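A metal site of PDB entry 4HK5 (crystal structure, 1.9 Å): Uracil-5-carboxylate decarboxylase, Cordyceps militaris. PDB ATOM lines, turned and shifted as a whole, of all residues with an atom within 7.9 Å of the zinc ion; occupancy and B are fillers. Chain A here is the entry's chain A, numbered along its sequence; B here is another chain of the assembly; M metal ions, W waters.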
ATOM      1  N   HIS A  15      -2.519  12.300  22.861  1.00  0.00           N
ATOM      2  CA  HIS A  15      -3.010  13.170  23.918  1.00  0.00           C
ATOM      3  C   HIS A  15      -3.040  14.566  23.393  1.00  0.00           C
ATOM      4  O   HIS A  15      -2.068  15.326  23.528  1.00  0.00           O
ATOM      5  CB  HIS A  15      -2.119  13.067  25.164  1.00  0.00           C
ATOM      6  CG  HIS A  15      -2.695  13.708  26.398  1.00  0.00           C
ATOM      7  ND1 HIS A  15      -2.382  13.286  27.646  1.00  0.00           N
ATOM      8  CD2 HIS A  15      -3.579  14.774  26.560  1.00  0.00           C
ATOM      9  CE1 HIS A  15      -3.036  14.043  28.547  1.00  0.00           C
ATOM     10  NE2 HIS A  15      -3.768  14.953  27.893  1.00  0.00           N
ATOM     11  N   THR A  16      -4.155  14.926  22.783  1.00  0.00           N
ATOM     12  CA  THR A  16      -4.291  16.173  22.046  1.00  0.00           C
ATOM     13  C   THR A  16      -5.781  16.522  21.930  1.00  0.00           C
ATOM     14  O   THR A  16      -6.611  15.635  21.678  1.00  0.00           O
ATOM     15  CB  THR A  16      -3.575  16.083  20.668  1.00  0.00           C
ATOM     16  OG1 THR A  16      -3.763  17.285  19.913  1.00  0.00           O
ATOM     17  CG2 THR A  16      -4.029  14.877  19.857  1.00  0.00           C
ATOM     18  N   HIS A  17      -6.108  17.794  22.129  1.00  0.00           N
ATOM     19  CA  HIS A  17      -7.488  18.188  22.409  1.00  0.00           C
ATOM     20  C   HIS A  17      -8.034  19.240  21.478  1.00  0.00           C
ATOM     21  O   HIS A  17      -7.288  20.019  20.893  1.00  0.00           O
ATOM     22  CB  HIS A  17      -7.598  18.722  23.830  1.00  0.00           C
ATOM     23  CG  HIS A  17      -7.150  17.743  24.886  1.00  0.00           C
ATOM     24  ND1 HIS A  17      -7.711  16.525  25.048  1.00  0.00           N
ATOM     25  CD2 HIS A  17      -6.183  17.858  25.886  1.00  0.00           C
ATOM     26  CE1 HIS A  17      -7.121  15.890  26.078  1.00  0.00           C
ATOM     27  NE2 HIS A  17      -6.203  16.709  26.598  1.00  0.00           N
ATOM     28  N   SER A  98      -9.160  14.412  21.138  1.00  0.00           N
ATOM     29  CA  SER A  98     -10.257  14.176  22.077  1.00  0.00           C
ATOM     30  C   SER A  98     -10.806  15.518  22.552  1.00  0.00           C
ATOM     31  O   SER A  98     -10.092  16.518  22.592  1.00  0.00           O
ATOM     32  CB  SER A  98      -9.783  13.340  23.267  1.00  0.00           C
ATOM     33  OG  SER A  98      -8.614  13.888  23.852  1.00  0.00           O
ATOM     34  N   LEU A  99     -12.081  15.530  22.907  1.00  0.00           N
ATOM     35  CA  LEU A  99     -12.669  16.667  23.584  1.00  0.00           C
ATOM     36  C   LEU A  99     -11.910  16.840  24.901  1.00  0.00           C
ATOM     37  O   LEU A  99     -11.585  15.858  25.567  1.00  0.00           O
ATOM     38  CB  LEU A  99     -14.156  16.432  23.846  1.00  0.00           C
ATOM     39  CG  LEU A  99     -14.950  17.535  24.537  1.00  0.00           C
ATOM     40  CD1 LEU A  99     -14.989  18.809  23.695  1.00  0.00           C
ATOM     41  CD2 LEU A  99     -16.355  17.057  24.844  1.00  0.00           C
ATOM     42  N   ALA A 100     -11.602  18.080  25.248  1.00  0.00           N
ATOM     43  CA  ALA A 100     -10.875  18.360  26.480  1.00  0.00           C
ATOM     44  C   ALA A 100     -11.809  18.391  27.677  1.00  0.00           C
ATOM     45  O   ALA A 100     -13.011  18.593  27.535  1.00  0.00           O
ATOM     46  CB  ALA A 100     -10.094  19.660  26.365  1.00  0.00           C
ATOM     47  N   ASN A 101     -11.230  18.174  28.849  1.00  0.00           N
ATOM     48  CA  ASN A 101     -11.944  18.308  30.106  1.00  0.00           C
ATOM     49  C   ASN A 101     -12.719  19.633  30.121  1.00  0.00           C
ATOM     50  O   ASN A 101     -12.223  20.626  29.617  1.00  0.00           O
ATOM     51  CB  ASN A 101     -10.953  18.213  31.284  1.00  0.00           C
ATOM     52  CG  ASN A 101      -9.704  19.066  31.086  1.00  0.00           C
ATOM     53  OD1 ASN A 101      -8.903  18.852  30.164  1.00  0.00           O
ATOM     54  ND2 ASN A 101      -9.514  20.032  31.987  1.00  0.00           N
ATOM     55  N   TRP A 103     -15.653  17.873  29.329  1.00  0.00           N
ATOM     56  CA  TRP A 103     -16.554  17.062  28.525  1.00  0.00           C
ATOM     57  C   TRP A 103     -17.987  17.378  28.841  1.00  0.00           C
ATOM     58  O   TRP A 103     -18.329  18.550  29.022  1.00  0.00           O
ATOM     59  CB  TRP A 103     -16.230  15.575  28.718  1.00  0.00           C
ATOM     60  CG  TRP A 103     -14.739  15.299  28.711  1.00  0.00           C
ATOM     61  CD1 TRP A 103     -13.901  15.213  27.621  1.00  0.00           C
ATOM     62  CD2 TRP A 103     -13.859  15.086  29.886  1.00  0.00           C
ATOM     63  NE1 TRP A 103     -12.606  14.962  28.002  1.00  0.00           N
ATOM     64  CE2 TRP A 103     -12.508  14.877  29.344  1.00  0.00           C
ATOM     65  CE3 TRP A 103     -14.044  15.048  31.258  1.00  0.00           C
ATOM     66  CZ2 TRP A 103     -11.424  14.640  30.163  1.00  0.00           C
ATOM     67  CZ3 TRP A 103     -12.943  14.811  32.076  1.00  0.00           C
ATOM     68  CH2 TRP A 103     -11.656  14.607  31.534  1.00  0.00           C
ATOM     69  N   ILE A 166     -12.784   8.792  25.593  1.00  0.00           N
ATOM     70  CA  ILE A 166     -12.140   9.544  26.674  1.00  0.00           C
ATOM     71  C   ILE A 166     -13.099   9.602  27.864  1.00  0.00           C
ATOM     72  O   ILE A 166     -14.299   9.874  27.701  1.00  0.00           O
ATOM     73  CB  ILE A 166     -11.638  10.944  26.235  1.00  0.00           C
ATOM     74  CG1 ILE A 166     -10.809  11.591  27.368  1.00  0.00           C
ATOM     75  CG2 ILE A 166     -12.788  11.839  25.751  1.00  0.00           C
ATOM     76  CD1 ILE A 166     -10.019  12.828  26.981  1.00  0.00           C
ATOM     77  N   PHE A 196      -9.346   6.148  27.349  1.00  0.00           N
ATOM     78  CA  PHE A 196      -8.351   7.147  27.716  1.00  0.00           C
ATOM     79  C   PHE A 196      -8.853   7.849  28.976  1.00  0.00           C
ATOM     80  O   PHE A 196      -9.787   8.646  28.917  1.00  0.00           O
ATOM     81  CB  PHE A 196      -8.151   8.116  26.540  1.00  0.00           C
ATOM     82  CG  PHE A 196      -7.162   9.222  26.787  1.00  0.00           C
ATOM     83  CD1 PHE A 196      -6.100   9.058  27.669  1.00  0.00           C
ATOM     84  CD2 PHE A 196      -7.276  10.422  26.089  1.00  0.00           C
ATOM     85  CE1 PHE A 196      -5.190  10.088  27.884  1.00  0.00           C
ATOM     86  CE2 PHE A 196      -6.367  11.445  26.292  1.00  0.00           C
ATOM     87  CZ  PHE A 196      -5.322  11.274  27.187  1.00  0.00           C
ATOM     88  N   HIS A 198      -8.564  10.508  31.937  1.00  0.00           N
ATOM     89  CA  HIS A 198      -8.009  11.862  31.947  1.00  0.00           C
ATOM     90  C   HIS A 198      -8.544  12.581  33.155  1.00  0.00           C
ATOM     91  O   HIS A 198      -9.734  12.453  33.479  1.00  0.00           O
ATOM     92  CB  HIS A 198      -8.416  12.575  30.649  1.00  0.00           C
ATOM     93  CG  HIS A 198      -7.713  13.894  30.415  1.00  0.00           C
ATOM     94  ND1 HIS A 198      -8.010  15.008  31.104  1.00  0.00           N
ATOM     95  CD2 HIS A 198      -6.710  14.242  29.517  1.00  0.00           C
ATOM     96  CE1 HIS A 198      -7.239  16.029  30.673  1.00  0.00           C
ATOM     97  NE2 HIS A 198      -6.444  15.557  29.699  1.00  0.00           N
ATOM     98  N   PRO A 199      -7.681  13.336  33.854  1.00  0.00           N
ATOM     99  CA  PRO A 199      -8.112  14.059  35.054  1.00  0.00           C
ATOM    100  C   PRO A 199      -8.918  15.323  34.714  1.00  0.00           C
ATOM    101  O   PRO A 199      -9.090  15.647  33.540  1.00  0.00           O
ATOM    102  CB  PRO A 199      -6.777  14.448  35.711  1.00  0.00           C
ATOM    103  CG  PRO A 199      -5.848  14.617  34.553  1.00  0.00           C
ATOM    104  CD  PRO A 199      -6.233  13.520  33.601  1.00  0.00           C
ATOM    105  N   PHE A 225      -3.705  17.268  38.929  1.00  0.00           N
ATOM    106  CA  PHE A 225      -4.125  16.397  37.833  1.00  0.00           C
ATOM    107  C   PHE A 225      -3.530  14.980  37.944  1.00  0.00           C
ATOM    108  O   PHE A 225      -4.280  14.005  38.007  1.00  0.00           O
ATOM    109  CB  PHE A 225      -3.764  17.038  36.475  1.00  0.00           C
ATOM    110  CG  PHE A 225      -4.838  17.932  35.904  1.00  0.00           C
ATOM    111  CD1 PHE A 225      -5.905  18.369  36.675  1.00  0.00           C
ATOM    112  CD2 PHE A 225      -4.761  18.336  34.576  1.00  0.00           C
ATOM    113  CE1 PHE A 225      -6.887  19.190  36.139  1.00  0.00           C
ATOM    114  CE2 PHE A 225      -5.739  19.171  34.023  1.00  0.00           C
ATOM    115  CZ  PHE A 225      -6.804  19.595  34.819  1.00  0.00           C
ATOM    116  N   ALA A 253      -3.554   9.094  31.289  1.00  0.00           N
ATOM    117  CA  ALA A 253      -2.966  10.401  31.059  1.00  0.00           C
ATOM    118  C   ALA A 253      -1.745  10.640  31.935  1.00  0.00           C
ATOM    119  O   ALA A 253      -1.669  10.161  33.069  1.00  0.00           O
ATOM    120  CB  ALA A 253      -4.012  11.487  31.324  1.00  0.00           C
ATOM    121  N   HIS A 254      -0.780  11.379  31.383  1.00  0.00           N
ATOM    122  CA  HIS A 254       0.414  11.816  32.124  1.00  0.00           C
ATOM    123  C   HIS A 254       1.170  10.671  32.752  1.00  0.00           C
ATOM    124  O   HIS A 254       1.510  10.701  33.942  1.00  0.00           O
ATOM    125  CB  HIS A 254       0.042  12.880  33.160  1.00  0.00           C
ATOM    126  CG  HIS A 254      -0.897  13.937  32.621  1.00  0.00           C
ATOM    127  ND1 HIS A 254      -2.057  14.263  33.232  1.00  0.00           N
ATOM    128  CD2 HIS A 254      -0.817  14.748  31.477  1.00  0.00           C
ATOM    129  CE1 HIS A 254      -2.678  15.232  32.535  1.00  0.00           C
ATOM    130  NE2 HIS A 254      -1.916  15.527  31.462  1.00  0.00           N
ATOM    131  N   ASP A 300       0.478   7.136  28.579  1.00  0.00           N
ATOM    132  CA  ASP A 300       1.041   8.155  27.685  1.00  0.00           C
ATOM    133  C   ASP A 300       2.434   8.579  28.165  1.00  0.00           C
ATOM    134  O   ASP A 300       2.833   8.260  29.283  1.00  0.00           O
ATOM    135  CB  ASP A 300       0.069   9.323  27.421  1.00  0.00           C
ATOM    136  CG  ASP A 300       0.065  10.376  28.509  1.00  0.00           C
ATOM    137  OD1 ASP A 300       1.032  10.488  29.317  1.00  0.00           O
ATOM    138  OD2 ASP A 300      -0.933  11.147  28.530  1.00  0.00           O
ATOM    139  N   VAL A 302       3.469  11.774  28.362  1.00  0.00           N
ATOM    140  CA  VAL A 302       3.405  13.198  28.697  1.00  0.00           C
ATOM    141  C   VAL A 302       3.934  13.346  30.124  1.00  0.00           C
ATOM    142  O   VAL A 302       3.164  13.428  31.096  1.00  0.00           O
ATOM    143  CB  VAL A 302       1.975  13.767  28.553  1.00  0.00           C
ATOM    144  CG1 VAL A 302       1.964  15.279  28.762  1.00  0.00           C
ATOM    145  CG2 VAL A 302       1.414  13.443  27.167  1.00  0.00           C
ATOM    146  N   THR A 325       1.148  15.192  23.512  1.00  0.00           N
ATOM    147  CA  THR A 325       1.600  16.584  23.654  1.00  0.00           C
ATOM    148  C   THR A 325       0.756  17.428  24.600  1.00  0.00           C
ATOM    149  O   THR A 325       1.197  18.486  25.034  1.00  0.00           O
ATOM    150  CB  THR A 325       1.583  17.310  22.299  1.00  0.00           C
ATOM    151  OG1 THR A 325       0.237  17.333  21.798  1.00  0.00           O
ATOM    152  CG2 THR A 325       2.499  16.629  21.296  1.00  0.00           C
ATOM    153  N   ASP A 326      -0.469  16.983  24.861  1.00  0.00           N
ATOM    154  CA  ASP A 326      -1.459  17.796  25.579  1.00  0.00           C
ATOM    155  C   ASP A 326      -1.765  19.130  24.868  1.00  0.00           C
ATOM    156  O   ASP A 326      -2.175  20.096  25.507  1.00  0.00           O
ATOM    157  CB  ASP A 326      -1.059  18.032  27.037  1.00  0.00           C
ATOM    158  CG  ASP A 326      -2.240  17.964  28.005  1.00  0.00           C
ATOM    159  OD1 ASP A 326      -3.399  17.990  27.545  1.00  0.00           O
ATOM    160  OD2 ASP A 326      -1.994  17.878  29.215  1.00  0.00           O
ATOM    161  N   HIS A 327      -1.570  19.158  23.553  1.00  0.00           N
ATOM    162  CA  HIS A 327      -1.951  20.321  22.737  1.00  0.00           C
ATOM    163  C   HIS A 327      -3.425  20.564  22.900  1.00  0.00           C
ATOM    164  O   HIS A 327      -4.199  19.611  22.865  1.00  0.00           O
ATOM    165  CB  HIS A 327      -1.615  20.049  21.281  1.00  0.00           C
ATOM    166  CG  HIS A 327      -1.898  21.219  20.373  1.00  0.00           C
ATOM    167  ND1 HIS A 327      -2.996  21.288  19.605  1.00  0.00           N
ATOM    168  CD2 HIS A 327      -1.184  22.389  20.142  1.00  0.00           C
ATOM    169  CE1 HIS A 327      -2.999  22.436  18.911  1.00  0.00           C
ATOM    170  NE2 HIS A 327      -1.884  23.112  19.246  1.00  0.00           N
ATOM    171  N   PRO A 328      -3.858  21.824  23.070  1.00  0.00           N
ATOM    172  CA  PRO A 328      -3.120  23.073  22.980  1.00  0.00           C
ATOM    173  C   PRO A 328      -2.917  23.771  24.316  1.00  0.00           C
ATOM    174  O   PRO A 328      -2.852  24.994  24.371  1.00  0.00           O
ATOM    175  CB  PRO A 328      -4.059  23.923  22.137  1.00  0.00           C
ATOM    176  CG  PRO A 328      -5.429  23.482  22.579  1.00  0.00           C
ATOM    177  CD  PRO A 328      -5.304  22.084  23.143  1.00  0.00           C
ATOM    178  N   PHE A 329      -2.822  22.999  25.395  1.00  0.00           N
ATOM    179  CA  PHE A 329      -2.819  23.596  26.719  1.00  0.00           C
ATOM    180  C   PHE A 329      -1.547  24.276  27.172  1.00  0.00           C
ATOM    181  O   PHE A 329      -1.598  25.147  28.043  1.00  0.00           O
ATOM    182  CB  PHE A 329      -3.273  22.575  27.770  1.00  0.00           C
ATOM    183  CG  PHE A 329      -4.758  22.378  27.797  1.00  0.00           C
ATOM    184  CD1 PHE A 329      -5.573  23.261  28.496  1.00  0.00           C
ATOM    185  CD2 PHE A 329      -5.338  21.330  27.100  1.00  0.00           C
ATOM    186  CE1 PHE A 329      -6.949  23.074  28.512  1.00  0.00           C
ATOM    187  CE2 PHE A 329      -6.707  21.144  27.123  1.00  0.00           C
ATOM    188  CZ  PHE A 329      -7.510  22.020  27.826  1.00  0.00           C
ATOM    189  N   PHE A 330      -0.407  23.930  26.593  1.00  0.00           N
ATOM    190  CA  PHE A 330       0.850  24.531  27.038  1.00  0.00           C
ATOM    191  C   PHE A 330       1.624  25.242  25.922  1.00  0.00           C
ATOM    192  O   PHE A 330       2.715  24.811  25.543  1.00  0.00           O
ATOM    193  CB  PHE A 330       1.718  23.487  27.749  1.00  0.00           C
ATOM    194  CG  PHE A 330       1.074  22.914  28.980  1.00  0.00           C
ATOM    195  CD1 PHE A 330       1.222  23.527  30.213  1.00  0.00           C
ATOM    196  CD2 PHE A 330       0.306  21.748  28.907  1.00  0.00           C
ATOM    197  CE1 PHE A 330       0.629  23.002  31.362  1.00  0.00           C
ATOM    198  CE2 PHE A 330      -0.300  21.221  30.040  1.00  0.00           C
ATOM    199  CZ  PHE A 330      -0.129  21.841  31.267  1.00  0.00           C
ATOM    200  N   ARG B 265       7.355  17.502  35.152  1.00  0.00           N
ATOM    201  CA  ARG B 265       6.050  18.146  35.005  1.00  0.00           C
ATOM    202  C   ARG B 265       5.990  19.505  35.728  1.00  0.00           C
ATOM    203  O   ARG B 265       5.488  20.479  35.192  1.00  0.00           O
ATOM    204  CB  ARG B 265       4.920  17.227  35.485  1.00  0.00           C
ATOM    205  CG  ARG B 265       3.534  17.776  35.193  1.00  0.00           C
ATOM    206  CD  ARG B 265       2.405  16.910  35.732  1.00  0.00           C
ATOM    207  NE  ARG B 265       1.124  17.509  35.377  1.00  0.00           N
ATOM    208  CZ  ARG B 265       0.564  17.442  34.161  1.00  0.00           C
ATOM    209  NH1 ARG B 265       1.153  16.757  33.190  1.00  0.00           N
ATOM    210  NH2 ARG B 265      -0.589  18.060  33.932  1.00  0.00           N
HETATM  211 ZN    ZN M   1      -5.021  16.749  28.498  1.00  0.00          ZN
HETATM  212  O   HOH W   1      -6.045  18.680  29.218  1.00  0.00           O
HETATM  213  O   HOH W   2      -3.979  17.099  30.448  1.00  0.00           O
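N of His 17 is in hydrogen-bond range of O of His 327, 2.7 Å away. A ring nitrogen (ND1) of His 17 sits at hydrogen-bond distance from the side-chain hydroxyl (OG) of Ser 98 (3.0 Å). NE2 of His 254 is in hydrogen-bond range of OD2 of Asp 326, at 3.3 Å. OD2 of Asp 300 sits at hydrogen-bond distance from ND1 of His 15, 2.7 Å away. The backbone NH (N) of Thr 325 sits at hydrogen-bond distance from the backbone carbonyl oxygen (O) of His 15, 3.2 Å away.
Water W2 bridges the side-chain carboxylate of Asp 326 (2.5 Å) and a ring nitrogen (NE2) of His 254 (2.8 Å).
Within 4 Å of the zinc ion: His 15, His 17, His 198 and Asp 326.
The zinc ion is bound by NE2 of His 198 (2.2 Å), water W2 (2.2 Å), NE2 of His 17 (2.2 Å), OD1 of Asp 326 (2.3 Å), NE2 of His 15 (2.3 Å) and water W1 (2.3 Å). The zinc ion has six donor atoms within binding distance.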
